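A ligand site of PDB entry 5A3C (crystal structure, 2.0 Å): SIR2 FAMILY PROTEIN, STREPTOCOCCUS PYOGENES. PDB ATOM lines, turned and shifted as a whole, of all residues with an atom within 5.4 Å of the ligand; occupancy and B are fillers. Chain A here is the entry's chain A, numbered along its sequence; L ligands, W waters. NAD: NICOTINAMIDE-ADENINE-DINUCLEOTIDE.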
ATOM      1  N   ILE A  42       9.688  22.240  27.058  1.00  0.00           N
ATOM      2  CA  ILE A  42       9.422  23.569  26.526  1.00  0.00           C
ATOM      3  C   ILE A  42       7.931  23.770  26.367  1.00  0.00           C
ATOM      4  O   ILE A  42       7.226  22.955  25.771  1.00  0.00           O
ATOM      5  CB  ILE A  42      10.183  23.799  25.197  1.00  0.00           C
ATOM      6  CG1 ILE A  42      11.661  24.027  25.522  1.00  0.00           C
ATOM      7  CG2 ILE A  42       9.637  25.002  24.434  1.00  0.00           C
ATOM      8  CD1 ILE A  42      12.566  24.007  24.305  1.00  0.00           C
ATOM      9  N   GLY A  43       7.445  24.871  26.952  1.00  0.00           N
ATOM     10  CA  GLY A  43       6.056  25.223  26.899  1.00  0.00           C
ATOM     11  C   GLY A  43       5.833  26.554  26.217  1.00  0.00           C
ATOM     12  O   GLY A  43       6.760  27.160  25.696  1.00  0.00           O
ATOM     13  N   ALA A  44       4.597  27.022  26.292  1.00  0.00           N
ATOM     14  CA  ALA A  44       4.146  28.177  25.511  1.00  0.00           C
ATOM     15  C   ALA A  44       4.907  29.452  25.852  1.00  0.00           C
ATOM     16  O   ALA A  44       5.021  30.329  25.009  1.00  0.00           O
ATOM     17  CB  ALA A  44       2.650  28.379  25.682  1.00  0.00           C
ATOM     18  N   GLY A  45       5.449  29.543  27.050  1.00  0.00           N
ATOM     19  CA  GLY A  45       6.230  30.721  27.476  1.00  0.00           C
ATOM     20  C   GLY A  45       7.429  31.025  26.587  1.00  0.00           C
ATOM     21  O   GLY A  45       7.752  32.178  26.355  1.00  0.00           O
ATOM     22  N   SER A  47       7.749  30.399  23.302  1.00  0.00           N
ATOM     23  CA  SER A  47       7.256  31.023  22.079  1.00  0.00           C
ATOM     24  C   SER A  47       6.703  32.450  22.319  1.00  0.00           C
ATOM     25  O   SER A  47       6.955  33.361  21.525  1.00  0.00           O
ATOM     26  CB  SER A  47       6.231  30.122  21.403  1.00  0.00           C
ATOM     27  OG  SER A  47       6.888  29.009  20.786  1.00  0.00           O
ATOM     28  N   ALA A  48       6.016  32.644  23.441  1.00  0.00           N
ATOM     29  CA  ALA A  48       5.517  33.964  23.827  1.00  0.00           C
ATOM     30  C   ALA A  48       6.637  34.971  24.084  1.00  0.00           C
ATOM     31  O   ALA A  48       6.513  36.128  23.737  1.00  0.00           O
ATOM     32  CB  ALA A  48       4.595  33.871  25.037  1.00  0.00           C
ATOM     33  N   ALA A  49       7.748  34.488  24.650  1.00  0.00           N
ATOM     34  CA  ALA A  49       8.936  35.308  24.879  1.00  0.00           C
ATOM     35  C   ALA A  49       9.582  35.808  23.595  1.00  0.00           C
ATOM     36  O   ALA A  49      10.225  36.849  23.610  1.00  0.00           O
ATOM     37  CB  ALA A  49       9.965  34.570  25.725  1.00  0.00           C
ATOM     38  N   TYR A  54      -0.507  34.699  22.215  1.00  0.00           N
ATOM     39  CA  TYR A  54      -1.851  34.164  21.976  1.00  0.00           C
ATOM     40  C   TYR A  54      -2.959  35.066  22.545  1.00  0.00           C
ATOM     41  O   TYR A  54      -4.139  34.697  22.585  1.00  0.00           O
ATOM     42  CB  TYR A  54      -1.945  32.723  22.497  1.00  0.00           C
ATOM     43  CG  TYR A  54      -1.302  31.730  21.532  1.00  0.00           C
ATOM     44  CD1 TYR A  54       0.035  31.851  21.165  1.00  0.00           C
ATOM     45  CD2 TYR A  54      -2.031  30.666  20.991  1.00  0.00           C
ATOM     46  CE1 TYR A  54       0.633  30.973  20.285  1.00  0.00           C
ATOM     47  CE2 TYR A  54      -1.432  29.767  20.103  1.00  0.00           C
ATOM     48  CZ  TYR A  54      -0.104  29.933  19.757  1.00  0.00           C
ATOM     49  OH  TYR A  54       0.502  29.061  18.887  1.00  0.00           O
ATOM     50  N   LEU A  76      -5.983  30.853  22.368  1.00  0.00           N
ATOM     51  CA  LEU A  76      -6.071  29.470  22.848  1.00  0.00           C
ATOM     52  C   LEU A  76      -7.507  29.097  23.048  1.00  0.00           C
ATOM     53  O   LEU A  76      -7.952  28.029  22.634  1.00  0.00           O
ATOM     54  CB  LEU A  76      -5.318  29.271  24.169  1.00  0.00           C
ATOM     55  CG  LEU A  76      -5.445  27.850  24.725  1.00  0.00           C
ATOM     56  CD1 LEU A  76      -4.842  26.819  23.755  1.00  0.00           C
ATOM     57  CD2 LEU A  76      -4.821  27.748  26.121  1.00  0.00           C
ATOM     58  N   THR A 127       5.203  20.786  24.699  1.00  0.00           N
ATOM     59  CA  THR A 127       3.755  20.822  24.579  1.00  0.00           C
ATOM     60  C   THR A 127       3.353  21.804  23.493  1.00  0.00           C
ATOM     61  O   THR A 127       2.157  21.926  23.183  1.00  0.00           O
ATOM     62  CB  THR A 127       3.111  21.230  25.917  1.00  0.00           C
ATOM     63  OG1 THR A 127       3.822  22.333  26.468  1.00  0.00           O
ATOM     64  CG2 THR A 127       3.151  20.074  26.902  1.00  0.00           C
ATOM     65  N   ASN A 128       4.320  22.520  22.919  1.00  0.00           N
ATOM     66  CA  ASN A 128       4.034  23.446  21.813  1.00  0.00           C
ATOM     67  C   ASN A 128       3.754  22.705  20.517  1.00  0.00           C
ATOM     68  O   ASN A 128       4.339  21.650  20.249  1.00  0.00           O
ATOM     69  CB  ASN A 128       5.209  24.399  21.591  1.00  0.00           C
ATOM     70  CG  ASN A 128       5.403  25.370  22.740  1.00  0.00           C
ATOM     71  OD1 ASN A 128       4.518  25.533  23.576  1.00  0.00           O
ATOM     72  ND2 ASN A 128       6.536  26.057  22.752  1.00  0.00           N
ATOM     73  N   ALA A 129       2.858  23.272  19.721  1.00  0.00           N
ATOM     74  CA  ALA A 129       2.476  22.654  18.471  1.00  0.00           C
ATOM     75  C   ALA A 129       2.783  23.534  17.265  1.00  0.00           C
ATOM     76  O   ALA A 129       2.430  23.190  16.154  1.00  0.00           O
ATOM     77  CB  ALA A 129       0.995  22.265  18.525  1.00  0.00           C
ATOM     78  N   ASP A 130       3.500  24.636  17.487  1.00  0.00           N
ATOM     79  CA  ASP A 130       3.872  25.551  16.389  1.00  0.00           C
ATOM     80  C   ASP A 130       5.112  25.035  15.629  1.00  0.00           C
ATOM     81  O   ASP A 130       5.573  23.914  15.891  1.00  0.00           O
ATOM     82  CB  ASP A 130       4.068  26.989  16.914  1.00  0.00           C
ATOM     83  CG  ASP A 130       5.244  27.151  17.915  1.00  0.00           C
ATOM     84  OD1 ASP A 130       6.191  26.332  17.934  1.00  0.00           O
ATOM     85  OD2 ASP A 130       5.229  28.152  18.688  1.00  0.00           O
ATOM     86  N   GLN A 147       1.981  17.019  22.284  1.00  0.00           N
ATOM     87  CA  GLN A 147       0.648  17.580  21.972  1.00  0.00           C
ATOM     88  C   GLN A 147       0.341  17.696  20.470  1.00  0.00           C
ATOM     89  O   GLN A 147      -0.573  18.423  20.076  1.00  0.00           O
ATOM     90  CB  GLN A 147       0.505  18.966  22.625  1.00  0.00           C
ATOM     91  CG  GLN A 147       0.495  18.911  24.154  1.00  0.00           C
ATOM     92  CD  GLN A 147      -0.862  18.475  24.656  1.00  0.00           C
ATOM     93  OE1 GLN A 147      -1.275  17.335  24.434  1.00  0.00           O
ATOM     94  NE2 GLN A 147      -1.591  19.387  25.285  1.00  0.00           N
ATOM     95  N   TYR A 150       0.308  21.674  14.608  1.00  0.00           N
ATOM     96  CA  TYR A 150      -0.811  22.326  13.940  1.00  0.00           C
ATOM     97  C   TYR A 150      -0.843  22.044  12.445  1.00  0.00           C
ATOM     98  O   TYR A 150      -1.890  22.171  11.818  1.00  0.00           O
ATOM     99  CB  TYR A 150      -0.743  23.844  14.113  1.00  0.00           C
ATOM    100  CG  TYR A 150      -0.818  24.367  15.522  1.00  0.00           C
ATOM    101  CD1 TYR A 150      -1.753  23.873  16.448  1.00  0.00           C
ATOM    102  CD2 TYR A 150       0.025  25.403  15.926  1.00  0.00           C
ATOM    103  CE1 TYR A 150      -1.825  24.400  17.741  1.00  0.00           C
ATOM    104  CE2 TYR A 150      -0.043  25.931  17.205  1.00  0.00           C
ATOM    105  CZ  TYR A 150      -0.963  25.434  18.100  1.00  0.00           C
ATOM    106  OH  TYR A 150      -0.990  25.969  19.361  1.00  0.00           O
ATOM    107  N   GLY A 239       9.182  27.998  30.388  1.00  0.00           N
ATOM    108  CA  GLY A 239       7.901  28.579  30.010  1.00  0.00           C
ATOM    109  C   GLY A 239       6.733  27.609  30.094  1.00  0.00           C
ATOM    110  O   GLY A 239       5.831  27.610  29.234  1.00  0.00           O
ATOM    111  N   VAL A 240       6.750  26.784  31.123  1.00  0.00           N
ATOM    112  CA  VAL A 240       5.695  25.793  31.342  1.00  0.00           C
ATOM    113  C   VAL A 240       4.861  26.235  32.529  1.00  0.00           C
ATOM    114  O   VAL A 240       5.401  26.462  33.611  1.00  0.00           O
ATOM    115  CB  VAL A 240       6.263  24.404  31.645  1.00  0.00           C
ATOM    116  CG1 VAL A 240       5.135  23.411  31.865  1.00  0.00           C
ATOM    117  CG2 VAL A 240       7.192  23.947  30.523  1.00  0.00           C
ATOM    118  N   GLY A 241       3.553  26.310  32.340  1.00  0.00           N
ATOM    119  CA  GLY A 241       2.643  26.780  33.387  1.00  0.00           C
ATOM    120  C   GLY A 241       1.666  25.730  33.886  1.00  0.00           C
ATOM    121  O   GLY A 241       2.030  24.561  34.074  1.00  0.00           O
ATOM    122  N   HIS A 242       0.412  26.153  34.095  1.00  0.00           N
ATOM    123  CA  HIS A 242      -0.617  25.335  34.723  1.00  0.00           C
ATOM    124  C   HIS A 242      -1.742  24.915  33.783  1.00  0.00           C
ATOM    125  O   HIS A 242      -2.651  24.217  34.205  1.00  0.00           O
ATOM    126  CB  HIS A 242      -1.233  26.076  35.927  1.00  0.00           C
ATOM    127  CG  HIS A 242      -0.867  25.511  37.268  1.00  0.00           C
ATOM    128  ND1 HIS A 242       0.272  24.760  37.484  1.00  0.00           N
ATOM    129  CD2 HIS A 242      -1.485  25.610  38.475  1.00  0.00           C
ATOM    130  CE1 HIS A 242       0.327  24.408  38.761  1.00  0.00           C
ATOM    131  NE2 HIS A 242      -0.722  24.907  39.385  1.00  0.00           N
ATOM    132  N   THR A 243      -1.676  25.293  32.512  1.00  0.00           N
ATOM    133  CA  THR A 243      -2.681  24.823  31.577  1.00  0.00           C
ATOM    134  C   THR A 243      -2.708  23.281  31.446  1.00  0.00           C
ATOM    135  O   THR A 243      -3.771  22.696  31.435  1.00  0.00           O
ATOM    136  CB  THR A 243      -2.495  25.471  30.199  1.00  0.00           C
ATOM    137  OG1 THR A 243      -2.366  26.889  30.366  1.00  0.00           O
ATOM    138  CG2 THR A 243      -3.685  25.160  29.294  1.00  0.00           C
ATOM    139  N   THR A 244      -1.559  22.615  31.334  1.00  0.00           N
ATOM    140  CA  THR A 244      -1.526  21.136  31.207  1.00  0.00           C
ATOM    141  C   THR A 244      -0.288  20.566  31.867  1.00  0.00           C
ATOM    142  O   THR A 244       0.556  19.960  31.204  1.00  0.00           O
ATOM    143  CB  THR A 244      -1.575  20.630  29.725  1.00  0.00           C
ATOM    144  OG1 THR A 244      -0.459  21.148  28.962  1.00  0.00           O
ATOM    145  CG2 THR A 244      -2.904  20.980  29.034  1.00  0.00           C
ATOM    146  N   PHE A 247       1.878  16.947  31.462  1.00  0.00           N
ATOM    147  CA  PHE A 247       2.770  16.521  30.381  1.00  0.00           C
ATOM    148  C   PHE A 247       4.248  16.738  30.632  1.00  0.00           C
ATOM    149  O   PHE A 247       5.044  15.838  30.347  1.00  0.00           O
ATOM    150  CB  PHE A 247       2.338  17.115  29.035  1.00  0.00           C
ATOM    151  CG  PHE A 247       1.021  16.576  28.582  1.00  0.00           C
ATOM    152  CD1 PHE A 247       0.869  15.209  28.351  1.00  0.00           C
ATOM    153  CD2 PHE A 247      -0.091  17.399  28.472  1.00  0.00           C
ATOM    154  CE1 PHE A 247      -0.354  14.676  27.970  1.00  0.00           C
ATOM    155  CE2 PHE A 247      -1.314  16.878  28.083  1.00  0.00           C
ATOM    156  CZ  PHE A 247      -1.446  15.515  27.843  1.00  0.00           C
ATOM    157  N   LEU A 267      12.583  28.031  34.188  1.00  0.00           N
ATOM    158  CA  LEU A 267      12.688  29.396  33.706  1.00  0.00           C
ATOM    159  C   LEU A 267      11.246  29.837  33.558  1.00  0.00           C
ATOM    160  O   LEU A 267      10.563  29.408  32.629  1.00  0.00           O
ATOM    161  CB  LEU A 267      13.389  29.458  32.349  1.00  0.00           C
ATOM    162  CG  LEU A 267      14.919  29.371  32.271  1.00  0.00           C
ATOM    163  CD1 LEU A 267      15.480  28.210  33.077  1.00  0.00           C
ATOM    164  CD2 LEU A 267      15.367  29.290  30.817  1.00  0.00           C
ATOM    165  N   ASN A 268      10.797  30.680  34.481  1.00  0.00           N
ATOM    166  CA  ASN A 268       9.425  31.146  34.494  1.00  0.00           C
ATOM    167  C   ASN A 268       9.343  32.443  35.296  1.00  0.00           C
ATOM    168  O   ASN A 268       9.824  32.493  36.418  1.00  0.00           O
ATOM    169  CB  ASN A 268       8.527  30.067  35.119  1.00  0.00           C
ATOM    170  CG  ASN A 268       7.099  30.137  34.615  1.00  0.00           C
ATOM    171  OD1 ASN A 268       6.421  31.139  34.759  1.00  0.00           O
ATOM    172  ND2 ASN A 268       6.644  29.056  34.013  1.00  0.00           N
ATOM    173  N   HIS A 269       8.718  33.486  34.750  1.00  0.00           N
ATOM    174  CA  HIS A 269       8.630  34.734  35.527  1.00  0.00           C
ATOM    175  C   HIS A 269       7.533  34.689  36.606  1.00  0.00           C
ATOM    176  O   HIS A 269       7.368  35.645  37.356  1.00  0.00           O
ATOM    177  CB  HIS A 269       8.538  35.997  34.639  1.00  0.00           C
ATOM    178  CG  HIS A 269       7.382  36.016  33.691  1.00  0.00           C
ATOM    179  ND1 HIS A 269       7.344  36.860  32.597  1.00  0.00           N
ATOM    180  CD2 HIS A 269       6.229  35.308  33.658  1.00  0.00           C
ATOM    181  CE1 HIS A 269       6.213  36.676  31.940  1.00  0.00           C
ATOM    182  NE2 HIS A 269       5.515  35.733  32.559  1.00  0.00           N
ATOM    183  N   LYS A 270       6.800  33.574  36.682  1.00  0.00           N
ATOM    184  CA  LYS A 270       5.875  33.280  37.777  1.00  0.00           C
ATOM    185  C   LYS A 270       6.360  32.092  38.612  1.00  0.00           C
ATOM    186  O   LYS A 270       6.984  31.155  38.084  1.00  0.00           O
ATOM    187  CB  LYS A 270       4.480  32.984  37.224  1.00  0.00           C
ATOM    188  CG  LYS A 270       3.804  34.197  36.622  1.00  0.00           C
ATOM    189  CD  LYS A 270       2.298  34.005  36.510  1.00  0.00           C
ATOM    190  CE  LYS A 270       1.585  35.343  36.297  1.00  0.00           C
ATOM    191  NZ  LYS A 270       0.121  35.231  36.590  1.00  0.00           N
ATOM    192  N   TYR A 272       5.722  28.795  40.694  1.00  0.00           N
ATOM    193  CA  TYR A 272       4.827  27.641  40.906  1.00  0.00           C
ATOM    194  C   TYR A 272       5.413  26.786  42.026  1.00  0.00           C
ATOM    195  O   TYR A 272       6.582  26.407  41.992  1.00  0.00           O
ATOM    196  CB  TYR A 272       4.677  26.811  39.631  1.00  0.00           C
ATOM    197  CG  TYR A 272       3.957  27.534  38.521  1.00  0.00           C
ATOM    198  CD1 TYR A 272       4.642  28.454  37.713  1.00  0.00           C
ATOM    199  CD2 TYR A 272       2.610  27.319  38.264  1.00  0.00           C
ATOM    200  CE1 TYR A 272       3.993  29.125  36.689  1.00  0.00           C
ATOM    201  CE2 TYR A 272       1.961  27.990  37.240  1.00  0.00           C
ATOM    202  CZ  TYR A 272       2.659  28.901  36.458  1.00  0.00           C
ATOM    203  OH  TYR A 272       2.043  29.579  35.443  1.00  0.00           O
ATOM    204  N   THR A 286      13.658  33.732  37.227  1.00  0.00           N
ATOM    205  CA  THR A 286      12.500  34.541  36.889  1.00  0.00           C
ATOM    206  C   THR A 286      12.685  35.528  35.745  1.00  0.00           C
ATOM    207  O   THR A 286      11.706  36.105  35.286  1.00  0.00           O
ATOM    208  CB  THR A 286      12.062  35.349  38.109  1.00  0.00           C
ATOM    209  OG1 THR A 286      13.201  36.001  38.667  1.00  0.00           O
ATOM    210  CG2 THR A 286      11.424  34.444  39.144  1.00  0.00           C
ATOM    211  N   GLU A 287      13.908  35.742  35.281  1.00  0.00           N
ATOM    212  CA  GLU A 287      14.147  36.718  34.212  1.00  0.00           C
ATOM    213  C   GLU A 287      13.471  36.329  32.895  1.00  0.00           C
ATOM    214  O   GLU A 287      13.325  35.147  32.573  1.00  0.00           O
ATOM    215  CB  GLU A 287      15.654  36.943  34.007  1.00  0.00           C
ATOM    216  CG  GLU A 287      16.256  37.869  35.054  1.00  0.00           C
ATOM    217  CD  GLU A 287      17.780  37.872  35.056  1.00  0.00           C
ATOM    218  OE1 GLU A 287      18.388  37.627  33.992  1.00  0.00           O
ATOM    219  OE2 GLU A 287      18.356  38.127  36.143  1.00  0.00           O
ATOM    220  N   HIS A 288      13.051  37.337  32.142  1.00  0.00           N
ATOM    221  CA  HIS A 288      12.389  37.144  30.862  1.00  0.00           C
ATOM    222  C   HIS A 288      13.190  36.095  30.068  1.00  0.00           C
ATOM    223  O   HIS A 288      14.398  36.215  29.929  1.00  0.00           O
ATOM    224  CB  HIS A 288      12.308  38.499  30.141  1.00  0.00           C
ATOM    225  CG  HIS A 288      11.489  38.487  28.885  1.00  0.00           C
ATOM    226  ND1 HIS A 288      11.878  37.819  27.749  1.00  0.00           N
ATOM    227  CD2 HIS A 288      10.345  39.136  28.556  1.00  0.00           C
ATOM    228  CE1 HIS A 288      11.001  38.020  26.782  1.00  0.00           C
ATOM    229  NE2 HIS A 288      10.054  38.814  27.257  1.00  0.00           N
ATOM    230  N   ILE A 289      12.503  35.043  29.627  1.00  0.00           N
ATOM    231  CA  ILE A 289      13.153  33.894  28.979  1.00  0.00           C
ATOM    232  C   ILE A 289      14.085  34.291  27.821  1.00  0.00           C
ATOM    233  O   ILE A 289      15.196  33.792  27.717  1.00  0.00           O
ATOM    234  CB  ILE A 289      12.104  32.891  28.478  1.00  0.00           C
ATOM    235  CG1 ILE A 289      11.591  32.047  29.647  1.00  0.00           C
ATOM    236  CG2 ILE A 289      12.673  31.978  27.390  1.00  0.00           C
ATOM    237  CD1 ILE A 289      10.216  31.462  29.382  1.00  0.00           C
ATOM    238  N   ALA A 290      13.607  35.157  26.931  1.00  0.00           N
ATOM    239  CA  ALA A 290      14.409  35.552  25.780  1.00  0.00           C
ATOM    240  C   ALA A 290      15.740  36.176  26.209  1.00  0.00           C
ATOM    241  O   ALA A 290      16.795  35.763  25.729  1.00  0.00           O
ATOM    242  CB  ALA A 290      13.638  36.487  24.872  1.00  0.00           C
HETATM  243  PA  NAD L   1       0.957  28.170  29.877  1.00  0.00           P
HETATM  244  O1A NAD L   1       0.409  29.328  29.134  1.00  0.00           O
HETATM  245  O2A NAD L   1       0.137  27.284  30.764  1.00  0.00           O
HETATM  246  O5B NAD L   1       2.180  28.690  30.745  1.00  0.00           O
HETATM  247  C5B NAD L   1       3.181  29.516  30.145  1.00  0.00           C
HETATM  248  C4B NAD L   1       4.174  29.882  31.237  1.00  0.00           C
HETATM  249  O4B NAD L   1       5.251  30.647  30.696  1.00  0.00           O
HETATM  250  C3B NAD L   1       3.505  30.728  32.317  1.00  0.00           C
HETATM  251  O3B NAD L   1       3.805  30.155  33.595  1.00  0.00           O
HETATM  252  C2B NAD L   1       4.119  32.111  32.160  1.00  0.00           C
HETATM  253  O2B NAD L   1       4.328  32.756  33.412  1.00  0.00           O
HETATM  254  C1B NAD L   1       5.460  31.800  31.514  1.00  0.00           C
HETATM  255  N9A NAD L   1       6.000  32.872  30.667  1.00  0.00           N
HETATM  256  C8A NAD L   1       5.383  33.465  29.636  1.00  0.00           C
HETATM  257  N7A NAD L   1       6.184  34.381  29.061  1.00  0.00           N
HETATM  258  C5A NAD L   1       7.351  34.361  29.748  1.00  0.00           C
HETATM  259  C6A NAD L   1       8.646  35.078  29.689  1.00  0.00           C
HETATM  260  N6A NAD L   1       8.855  36.016  28.750  1.00  0.00           N
HETATM  261  N1A NAD L   1       9.612  34.763  30.584  1.00  0.00           N
HETATM  262  C2A NAD L   1       9.419  33.828  31.527  1.00  0.00           C
HETATM  263  N3A NAD L   1       8.250  33.139  31.638  1.00  0.00           N
HETATM  264  C4A NAD L   1       7.218  33.364  30.803  1.00  0.00           C
HETATM  265  O3  NAD L   1       1.741  27.291  28.764  1.00  0.00           O
HETATM  266  PN  NAD L   1       1.897  25.671  28.655  1.00  0.00           P
HETATM  267  O1N NAD L   1       2.341  25.087  29.975  1.00  0.00           O
HETATM  268  O2N NAD L   1       2.794  25.434  27.461  1.00  0.00           O
HETATM  269  O5D NAD L   1       0.435  25.103  28.299  1.00  0.00           O
HETATM  270  C5D NAD L   1      -0.292  25.528  27.159  1.00  0.00           C
HETATM  271  C4D NAD L   1      -1.124  24.385  26.631  1.00  0.00           C
HETATM  272  O4D NAD L   1      -1.892  24.844  25.524  1.00  0.00           O
HETATM  273  C3D NAD L   1      -0.233  23.285  26.090  1.00  0.00           C
HETATM  274  O3D NAD L   1      -0.787  22.005  26.428  1.00  0.00           O
HETATM  275  C2D NAD L   1      -0.189  23.540  24.590  1.00  0.00           C
HETATM  276  O2D NAD L   1      -0.474  22.341  23.852  1.00  0.00           O
HETATM  277  C1D NAD L   1      -1.217  24.618  24.280  1.00  0.00           C
HETATM  278  N1N NAD L   1      -0.615  25.865  23.719  1.00  0.00           N
HETATM  279  C2N NAD L   1       0.348  25.796  22.761  1.00  0.00           C
HETATM  280  C3N NAD L   1       0.925  26.943  22.214  1.00  0.00           C
HETATM  281  C7N NAD L   1       2.014  26.846  21.159  1.00  0.00           C
HETATM  282  O7N NAD L   1       2.069  25.880  20.414  1.00  0.00           O
HETATM  283  N7N NAD L   1       2.940  27.820  21.057  1.00  0.00           N
HETATM  284  C4N NAD L   1       0.482  28.185  22.674  1.00  0.00           C
HETATM  285  C5N NAD L   1      -0.508  28.240  23.653  1.00  0.00           C
HETATM  286  C6N NAD L   1      -1.048  27.062  24.160  1.00  0.00           C
HETATM  287  O   HOH W   1       3.366  22.259  29.229  1.00  0.00           O
HETATM  288  O   HOH W   2      12.011  32.785  33.385  1.00  0.00           O
HETATM  289  O   HOH W   3       1.016  23.317  31.428  1.00  0.00           O
HETATM  290  O   HOH W   4      -3.392  22.571  25.067  1.00  0.00           O
HETATM  291  O   HOH W   5       2.977  24.423  25.235  1.00  0.00           O
HETATM  292  O   HOH W   6       6.563  36.635  27.334  1.00  0.00           O
HETATM  293  O   HOH W   7       2.813  30.883  22.629  1.00  0.00           O
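A ring nitrogen (NE2) of His 269 lies close to an oxygen (O2B) of the ligand, at 3.3 Å. An oxygen (O7N) of the ligand is in hydrogen-bond range of the backbone NH of Asp 130, at 3.5 Å. An oxygen (O2A) of the ligand sits at hydrogen-bond distance from the backbone NH (N) of Thr 243, 3.2 Å away. An oxygen (O7N) of the ligand lies within hydrogen-bond range of the side-chain hydroxyl (OH) of Tyr 150 (3.2 Å). The backbone NH (N) of Ala 129 is in hydrogen-bond range of an oxygen (O7N) of the ligand (2.8 Å). O of Thr 127 sits at hydrogen-bond distance from O2D of the ligand, 2.7 Å away. The side-chain hydroxyl (OH) of Tyr 54 sits at hydrogen-bond distance from a nitrogen (N7N) of the ligand, 3.5 Å away. N of His 269 is in hydrogen-bond range of N3A of the ligand (3.2 Å). An oxygen (O3D) of the ligand sits at hydrogen-bond distance from the side-chain amide nitrogen (NE2) of Gln 147 (3.0 Å). N7N of the ligand sits at hydrogen-bond distance from OD2 of Asp 130. The side-chain hydroxyl of Thr 243 lies within hydrogen-bond range of an oxygen (O2A) of the ligand (2.6 Å). An oxygen (O1N) of the ligand sits at hydrogen-bond distance from the backbone NH of Gly 241 (2.9 Å). The backbone NH of Ile 289 lies within hydrogen-bond range of a nitrogen (N1A) of the ligand, at 3.1 Å. OD1 of Asn 268 sits at hydrogen-bond distance from O2B of the ligand, 3.0 Å away. O2N of the ligand is in hydrogen-bond range of N of Ala 44, at 2.7 Å. A nitrogen (N6A) of the ligand lies within hydrogen-bond range of a ring nitrogen (NE2) of His 288, at 3.4 Å. An oxygen (O3D) of the ligand sits at hydrogen-bond distance from the side-chain hydroxyl (OG1) of Thr 244 (2.7 Å). An oxygen (O3B) of the ligand sits at hydrogen-bond distance from the side-chain hydroxyl (OH) of Tyr 272, at 2.6 Å. The side-chain hydroxyl (OG1) of Thr 127 lies within hydrogen-bond range of an oxygen (O2N) of the ligand (3.4 Å).
The backbone carbonyl oxygen (O) of Ile 42 is in hydrogen-bond range of the backbone NH (N) of Thr 127, at 3.2 Å. The side-chain amide nitrogen (ND2) of Asn 268 is in hydrogen-bond range of the backbone carbonyl oxygen (O) of Val 240, at 2.9 Å. OH of Tyr 54 is in hydrogen-bond range of OH of Tyr 150 (3.5 Å). The side-chain hydroxyl (OG) of Ser 47 is in hydrogen-bond range of the side-chain carboxylate (OD2) of Asp 130, at 2.8 Å. The backbone NH (N) of Tyr 150 is in hydrogen-bond range of the backbone carbonyl oxygen (O) of Ala 129 (3.0 Å). The side-chain amide oxygen of Asn 268 sits close to the backbone NH of Lys 270. O of Leu 267 is in hydrogen-bond range of N of Gly 239 (3.0 Å). N of Ala 44 is in hydrogen-bond range of OD1 of Asn 128 (3.1 Å).
The backbone carbonyl oxygen (O) of Gly 239 lies close to an oxygen (O4B) of the ligand, at 3.4 Å. Merely in contact with the ligand: Gly 43 (3.3 Å), Gly 45 (3.4 Å), Asn 128 (3.4 Å), His 242 (3.5 Å), Ala 49 (3.5 Å), Lys 270 (3.6 Å), Val 240 (3.7 Å) and Leu 76 (3.8 Å). Hydrophobic or aromatic side chains that line the ligand: Ala 44, Ala 49, Tyr 54, Leu 76, Tyr 150, Val 240, His 269, Tyr 272, His 288 and Ile 289. 24 residues have an atom within 4 Å of the ligand: Gly 43, Ala 44, Gly 45, Ala 49, Tyr 54, Leu 76, Thr 127, Asn 128, Ala 129, Asp 130, Gln 147, Tyr 150, Gly 239, Val 240, Gly 241, His 242, Thr 243, Thr 244, Asn 268, His 269, Lys 270, Tyr 272, His 288 and Ile 289. Along chain A the residues within 4 Å of the ligand span positions 43 to 289.
Water W5 lies within hydrogen-bond range of an oxygen (O2N) of the ligand (2.5 Å), the side-chain amide oxygen (OD1) of Asn 128 (2.5 Å), the side-chain hydroxyl (OG1) of Thr 127 (2.6 Å) and the backbone NH (N) of Ala 44 (3.2 Å). Water W3 lies within hydrogen-bond range of an oxygen (O1N) of the ligand (2.6 Å), the backbone NH of Thr 244 (2.7 Å) and the backbone carbonyl oxygen of Gly 241 (3.1 Å). Water W1 lies within hydrogen-bond range of the side-chain hydroxyl (OG1) of Thr 127 (2.8 Å) and an oxygen (O1N) of the ligand (3.1 Å). Water W2 lies within hydrogen-bond range of N of Asn 268 (2.7 Å) and O of Glu 287 (2.8 Å). Water W7 bridges the backbone carbonyl oxygen (O) of Ala 44 (3.3 Å) and a nitrogen (N7N) of the ligand (3.4 Å).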
